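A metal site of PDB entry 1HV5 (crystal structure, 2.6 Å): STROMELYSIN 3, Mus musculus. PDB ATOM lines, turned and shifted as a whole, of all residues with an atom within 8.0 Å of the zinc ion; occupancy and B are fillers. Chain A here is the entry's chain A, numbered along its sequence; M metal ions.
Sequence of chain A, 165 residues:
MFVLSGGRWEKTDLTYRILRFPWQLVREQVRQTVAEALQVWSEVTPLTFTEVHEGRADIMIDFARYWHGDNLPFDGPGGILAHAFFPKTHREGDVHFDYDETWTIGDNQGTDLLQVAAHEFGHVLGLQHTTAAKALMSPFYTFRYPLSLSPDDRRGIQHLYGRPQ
Leu 72 touches the zinc ion.
CE2 of Phe 85 touches the zinc ion, at 3.99 Å.
Of the 21 residues printed, 6 come within 4 Å of the zinc ion.
Along chain A the residues within 4 Å of the zinc ion span positions 68 to 96.
N of Leu 72 is in hydrogen-bond range of OD1 of Asp 70, at 2.9 Å.
A ring nitrogen (ND1) of His 68 is in hydrogen-bond range of the backbone carbonyl oxygen of Tyr 66, at 2.5 Å.
N of Phe 85 lies within hydrogen-bond range of O of Asp 94 (2.8 Å).
OD2 of Asp 70 is bound to the zinc ion, at 2.1 Å.
NE2 of His 68 is bound to the zinc ion, 2.2 Å away.
The zinc ion is bound by a ring nitrogen (ND1) of His 96 (2.2 Å).
The zinc ion is bound by NE2 of His 83 (2.4 Å).
The zinc ion has four donor atoms within binding distance.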
ATOM      1  N   ASP A  62     -24.607  16.579   1.556  1.00  0.00           N
ATOM      2  CA  ASP A  62     -25.505  17.362   2.379  1.00  0.00           C
ATOM      3  C   ASP A  62     -24.973  17.523   3.816  1.00  0.00           C
ATOM      4  O   ASP A  62     -24.201  16.706   4.317  1.00  0.00           O
ATOM      5  CB  ASP A  62     -26.886  16.712   2.410  1.00  0.00           C
ATOM      6  CG  ASP A  62     -27.988  17.694   2.789  1.00  0.00           C
ATOM      7  OD1 ASP A  62     -27.718  18.954   2.903  1.00  0.00           O
ATOM      8  OD2 ASP A  62     -29.182  17.265   2.998  1.00  0.00           O
ATOM      9  N   ALA A  64     -26.561  17.801   7.373  1.00  0.00           N
ATOM     10  CA  ALA A  64     -27.798  17.559   8.136  1.00  0.00           C
ATOM     11  C   ALA A  64     -27.498  17.294   9.606  1.00  0.00           C
ATOM     12  O   ALA A  64     -26.354  17.065  10.002  1.00  0.00           O
ATOM     13  CB  ALA A  64     -28.522  16.339   7.564  1.00  0.00           C
ATOM     14  N   ARG A  65     -28.580  17.334  10.386  1.00  0.00           N
ATOM     15  CA  ARG A  65     -28.488  17.100  11.819  1.00  0.00           C
ATOM     16  C   ARG A  65     -29.485  16.048  12.270  1.00  0.00           C
ATOM     17  O   ARG A  65     -30.647  16.025  11.819  1.00  0.00           O
ATOM     18  CB  ARG A  65     -28.746  18.391  12.617  1.00  0.00           C
ATOM     19  CG  ARG A  65     -29.955  19.189  12.153  1.00  0.00           C
ATOM     20  CD  ARG A  65     -29.918  20.648  12.630  1.00  0.00           C
ATOM     21  NE  ARG A  65     -30.426  20.818  14.003  1.00  0.00           N
ATOM     22  CZ  ARG A  65     -29.870  20.273  15.096  1.00  0.00           C
ATOM     23  NH1 ARG A  65     -28.781  19.499  15.005  1.00  0.00           N
ATOM     24  NH2 ARG A  65     -30.345  20.426  16.341  1.00  0.00           N
ATOM     25  N   TYR A  66     -28.937  15.236  13.137  1.00  0.00           N
ATOM     26  CA  TYR A  66     -29.642  14.147  13.801  1.00  0.00           C
ATOM     27  C   TYR A  66     -30.211  13.151  12.785  1.00  0.00           C
ATOM     28  O   TYR A  66     -29.550  12.845  11.771  1.00  0.00           O
ATOM     29  CB  TYR A  66     -30.753  14.753  14.650  1.00  0.00           C
ATOM     30  CG  TYR A  66     -30.216  15.333  15.952  1.00  0.00           C
ATOM     31  CD1 TYR A  66     -30.024  16.721  16.096  1.00  0.00           C
ATOM     32  CD2 TYR A  66     -29.907  14.473  17.008  1.00  0.00           C
ATOM     33  CE1 TYR A  66     -29.509  17.232  17.291  1.00  0.00           C
ATOM     34  CE2 TYR A  66     -29.377  14.975  18.195  1.00  0.00           C
ATOM     35  CZ  TYR A  66     -29.171  16.360  18.343  1.00  0.00           C
ATOM     36  OH  TYR A  66     -28.642  16.850  19.495  1.00  0.00           O
ATOM     37  N   TRP A  67     -31.412  12.664  13.154  1.00  0.00           N
ATOM     38  CA  TRP A  67     -32.417  12.272  11.900  1.00  0.00           C
ATOM     39  C   TRP A  67     -32.861  13.058  10.654  1.00  0.00           C
ATOM     40  O   TRP A  67     -33.690  13.979  10.742  1.00  0.00           O
ATOM     41  CB  TRP A  67     -33.686  11.814  12.684  1.00  0.00           C
ATOM     42  CG  TRP A  67     -33.538  10.485  13.467  1.00  0.00           C
ATOM     43  CD1 TRP A  67     -33.710   9.226  12.984  1.00  0.00           C
ATOM     44  CD2 TRP A  67     -33.188  10.357  14.844  1.00  0.00           C
ATOM     45  NE1 TRP A  67     -33.474   8.315  14.074  1.00  0.00           N
ATOM     46  CE2 TRP A  67     -33.174   8.998  15.151  1.00  0.00           C
ATOM     47  CE3 TRP A  67     -32.895  11.283  15.848  1.00  0.00           C
ATOM     48  CZ2 TRP A  67     -32.875   8.511  16.430  1.00  0.00           C
ATOM     49  CZ3 TRP A  67     -32.595  10.774  17.129  1.00  0.00           C
ATOM     50  CH2 TRP A  67     -32.587   9.452  17.410  1.00  0.00           C
ATOM     51  N   HIS A  68     -32.296  12.666   9.512  1.00  0.00           N
ATOM     52  CA  HIS A  68     -32.582  13.324   8.220  1.00  0.00           C
ATOM     53  C   HIS A  68     -33.045  12.309   7.162  1.00  0.00           C
ATOM     54  O   HIS A  68     -32.874  12.532   5.957  1.00  0.00           O
ATOM     55  CB  HIS A  68     -31.334  14.042   7.708  1.00  0.00           C
ATOM     56  CG  HIS A  68     -30.050  13.269   7.985  1.00  0.00           C
ATOM     57  ND1 HIS A  68     -29.655  12.954   9.267  1.00  0.00           N
ATOM     58  CD2 HIS A  68     -29.107  12.768   7.144  1.00  0.00           C
ATOM     59  CE1 HIS A  68     -28.517  12.281   9.187  1.00  0.00           C
ATOM     60  NE2 HIS A  68     -28.180  12.168   7.929  1.00  0.00           N
ATOM     61  N   GLY A  69     -33.594  11.220   7.675  1.00  0.00           N
ATOM     62  CA  GLY A  69     -34.248  10.178   6.869  1.00  0.00           C
ATOM     63  C   GLY A  69     -33.309   9.190   6.162  1.00  0.00           C
ATOM     64  O   GLY A  69     -33.410   8.929   4.954  1.00  0.00           O
ATOM     65  N   ASP A  70     -32.402   8.564   6.893  1.00  0.00           N
ATOM     66  CA  ASP A  70     -31.560   7.552   6.242  1.00  0.00           C
ATOM     67  C   ASP A  70     -31.102   6.460   7.204  1.00  0.00           C
ATOM     68  O   ASP A  70     -30.323   5.570   6.841  1.00  0.00           O
ATOM     69  CB  ASP A  70     -30.361   8.199   5.533  1.00  0.00           C
ATOM     70  CG  ASP A  70     -29.293   8.757   6.463  1.00  0.00           C
ATOM     71  OD1 ASP A  70     -29.479   8.758   7.736  1.00  0.00           O
ATOM     72  OD2 ASP A  70     -28.205   9.257   5.973  1.00  0.00           O
ATOM     73  N   ASN A  71     -31.597   6.532   8.427  1.00  0.00           N
ATOM     74  CA  ASN A  71     -31.329   5.502   9.443  1.00  0.00           C
ATOM     75  C   ASN A  71     -29.911   5.610  10.013  1.00  0.00           C
ATOM     76  O   ASN A  71     -29.412   4.689  10.676  1.00  0.00           O
ATOM     77  CB  ASN A  71     -31.490   4.121   8.829  1.00  0.00           C
ATOM     78  CG  ASN A  71     -32.931   3.851   8.399  1.00  0.00           C
ATOM     79  OD1 ASN A  71     -33.849   3.980   9.202  1.00  0.00           O
ATOM     80  ND2 ASN A  71     -33.181   3.478   7.151  1.00  0.00           N
ATOM     81  N   LEU A  72     -29.285   6.725   9.748  1.00  0.00           N
ATOM     82  CA  LEU A  72     -27.957   7.029  10.283  1.00  0.00           C
ATOM     83  C   LEU A  72     -28.034   8.405  10.910  1.00  0.00           C
ATOM     84  O   LEU A  72     -27.445   9.366  10.393  1.00  0.00           O
ATOM     85  CB  LEU A  72     -26.918   7.042   9.170  1.00  0.00           C
ATOM     86  CG  LEU A  72     -26.512   5.647   8.692  1.00  0.00           C
ATOM     87  CD1 LEU A  72     -25.206   5.668   7.885  1.00  0.00           C
ATOM     88  CD2 LEU A  72     -26.295   4.650   9.833  1.00  0.00           C
ATOM     89  N   PRO A  73     -28.745   8.557  12.033  1.00  0.00           N
ATOM     90  CA  PRO A  73     -28.922   9.851  12.655  1.00  0.00           C
ATOM     91  C   PRO A  73     -27.618  10.376  13.156  1.00  0.00           C
ATOM     92  O   PRO A  73     -26.797   9.560  13.673  1.00  0.00           O
ATOM     93  CB  PRO A  73     -29.767   9.570  13.879  1.00  0.00           C
ATOM     94  CG  PRO A  73     -29.984   8.068  13.940  1.00  0.00           C
ATOM     95  CD  PRO A  73     -29.377   7.432  12.727  1.00  0.00           C
ATOM     96  N   PHE A  74     -27.409  11.667  13.039  1.00  0.00           N
ATOM     97  CA  PHE A  74     -26.189  12.285  13.592  1.00  0.00           C
ATOM     98  C   PHE A  74     -26.433  12.497  15.097  1.00  0.00           C
ATOM     99  O   PHE A  74     -27.564  12.336  15.582  1.00  0.00           O
ATOM    100  CB  PHE A  74     -25.858  13.595  12.883  1.00  0.00           C
ATOM    101  CG  PHE A  74     -25.162  13.379  11.527  1.00  0.00           C
ATOM    102  CD1 PHE A  74     -24.047  12.534  11.419  1.00  0.00           C
ATOM    103  CD2 PHE A  74     -25.634  14.049  10.393  1.00  0.00           C
ATOM    104  CE1 PHE A  74     -23.418  12.361  10.172  1.00  0.00           C
ATOM    105  CE2 PHE A  74     -25.015  13.872   9.154  1.00  0.00           C
ATOM    106  CZ  PHE A  74     -23.906  13.025   9.038  1.00  0.00           C
ATOM    107  N   ALA A  82     -19.446  13.001  10.126  1.00  0.00           N
ATOM    108  CA  ALA A  82     -20.024  12.755   8.806  1.00  0.00           C
ATOM    109  C   ALA A  82     -19.980  11.268   8.498  1.00  0.00           C
ATOM    110  O   ALA A  82     -19.427  10.481   9.260  1.00  0.00           O
ATOM    111  CB  ALA A  82     -19.198  13.501   7.745  1.00  0.00           C
ATOM    112  N   HIS A  83     -20.597  10.932   7.402  1.00  0.00           N
ATOM    113  CA  HIS A  83     -20.623   9.562   6.902  1.00  0.00           C
ATOM    114  C   HIS A  83     -21.086   9.600   5.458  1.00  0.00           C
ATOM    115  O   HIS A  83     -21.659  10.592   5.001  1.00  0.00           O
ATOM    116  CB  HIS A  83     -21.538   8.683   7.778  1.00  0.00           C
ATOM    117  CG  HIS A  83     -22.976   9.182   7.905  1.00  0.00           C
ATOM    118  ND1 HIS A  83     -23.587   9.338   9.154  1.00  0.00           N
ATOM    119  CD2 HIS A  83     -23.899   9.559   6.986  1.00  0.00           C
ATOM    120  CE1 HIS A  83     -24.821   9.785   8.949  1.00  0.00           C
ATOM    121  NE2 HIS A  83     -25.015   9.918   7.662  1.00  0.00           N
ATOM    122  N   ALA A  84     -20.814   8.518   4.773  1.00  0.00           N
ATOM    123  CA  ALA A  84     -21.180   8.370   3.368  1.00  0.00           C
ATOM    124  C   ALA A  84     -21.710   6.969   3.160  1.00  0.00           C
ATOM    125  O   ALA A  84     -21.179   5.986   3.691  1.00  0.00           O
ATOM    126  CB  ALA A  84     -19.944   8.589   2.490  1.00  0.00           C
ATOM    127  N   PHE A  85     -22.773   6.877   2.389  1.00  0.00           N
ATOM    128  CA  PHE A  85     -23.393   5.575   2.125  1.00  0.00           C
ATOM    129  C   PHE A  85     -24.009   5.539   0.734  1.00  0.00           C
ATOM    130  O   PHE A  85     -24.313   6.578   0.140  1.00  0.00           O
ATOM    131  CB  PHE A  85     -24.467   5.290   3.174  1.00  0.00           C
ATOM    132  CG  PHE A  85     -25.677   6.193   3.033  1.00  0.00           C
ATOM    133  CD1 PHE A  85     -26.664   5.884   2.091  1.00  0.00           C
ATOM    134  CD2 PHE A  85     -25.800   7.328   3.841  1.00  0.00           C
ATOM    135  CE1 PHE A  85     -27.784   6.706   1.965  1.00  0.00           C
ATOM    136  CE2 PHE A  85     -26.925   8.149   3.706  1.00  0.00           C
ATOM    137  CZ  PHE A  85     -27.919   7.845   2.768  1.00  0.00           C
ATOM    138  N   ASP A  94     -23.860   9.036  -1.440  1.00  0.00           N
ATOM    139  CA  ASP A  94     -24.385  10.055  -0.528  1.00  0.00           C
ATOM    140  C   ASP A  94     -23.395  10.345   0.597  1.00  0.00           C
ATOM    141  O   ASP A  94     -22.903   9.428   1.264  1.00  0.00           O
ATOM    142  CB  ASP A  94     -25.706   9.598   0.072  1.00  0.00           C
ATOM    143  CG  ASP A  94     -26.860   9.802  -0.883  1.00  0.00           C
ATOM    144  OD1 ASP A  94     -28.074   9.602  -0.482  1.00  0.00           O
ATOM    145  OD2 ASP A  94     -26.632  10.174  -2.090  1.00  0.00           O
ATOM    146  N   VAL A  95     -23.137  11.619   0.765  1.00  0.00           N
ATOM    147  CA  VAL A  95     -22.227  12.080   1.828  1.00  0.00           C
ATOM    148  C   VAL A  95     -22.893  13.191   2.624  1.00  0.00           C
ATOM    149  O   VAL A  95     -23.307  14.226   2.067  1.00  0.00           O
ATOM    150  CB  VAL A  95     -20.928  12.596   1.244  1.00  0.00           C
ATOM    151  CG1 VAL A  95     -19.960  13.083   2.338  1.00  0.00           C
ATOM    152  CG2 VAL A  95     -20.168  11.533   0.452  1.00  0.00           C
ATOM    153  N   HIS A  96     -22.963  12.954   3.909  1.00  0.00           N
ATOM    154  CA  HIS A  96     -23.576  13.895   4.832  1.00  0.00           C
ATOM    155  C   HIS A  96     -22.607  14.276   5.943  1.00  0.00           C
ATOM    156  O   HIS A  96     -21.999  13.412   6.584  1.00  0.00           O
ATOM    157  CB  HIS A  96     -24.815  13.261   5.481  1.00  0.00           C
ATOM    158  CG  HIS A  96     -25.850  12.820   4.449  1.00  0.00           C
ATOM    159  ND1 HIS A  96     -26.866  11.913   4.767  1.00  0.00           N
ATOM    160  CD2 HIS A  96     -26.026  13.142   3.142  1.00  0.00           C
ATOM    161  CE1 HIS A  96     -27.598  11.722   3.685  1.00  0.00           C
ATOM    162  NE2 HIS A  96     -27.109  12.445   2.706  1.00  0.00           N
ATOM    163  N   PHE A  97     -22.479  15.571   6.109  1.00  0.00           N
ATOM    164  CA  PHE A  97     -21.671  16.160   7.182  1.00  0.00           C
ATOM    165  C   PHE A  97     -22.632  16.577   8.279  1.00  0.00           C
ATOM    166  O   PHE A  97     -23.728  17.088   7.983  1.00  0.00           O
ATOM    167  CB  PHE A  97     -20.936  17.392   6.678  1.00  0.00           C
ATOM    168  CG  PHE A  97     -19.907  17.058   5.619  1.00  0.00           C
ATOM    169  CD1 PHE A  97     -18.591  16.796   5.993  1.00  0.00           C
ATOM    170  CD2 PHE A  97     -20.290  17.021   4.280  1.00  0.00           C
ATOM    171  CE1 PHE A  97     -17.644  16.479   5.021  1.00  0.00           C
ATOM    172  CE2 PHE A  97     -19.351  16.693   3.304  1.00  0.00           C
ATOM    173  CZ  PHE A  97     -18.022  16.413   3.672  1.00  0.00           C
ATOM    174  N   ASP A  98     -22.233  16.356   9.518  1.00  0.00           N
ATOM    175  CA  ASP A  98     -23.081  16.728  10.656  1.00  0.00           C
ATOM    176  C   ASP A  98     -23.049  18.255  10.786  1.00  0.00           C
ATOM    177  O   ASP A  98     -22.029  18.846  11.101  1.00  0.00           O
ATOM    178  CB  ASP A  98     -22.555  16.104  11.953  1.00  0.00           C
ATOM    179  CG  ASP A  98     -23.517  16.267  13.118  1.00  0.00           C
ATOM    180  OD1 ASP A  98     -24.379  17.168  13.098  1.00  0.00           O
ATOM    181  OD2 ASP A  98     -23.403  15.493  14.084  1.00  0.00           O
HETATM  182 ZN    ZN M   1     -27.026  10.790   6.700  1.00  0.00          ZN
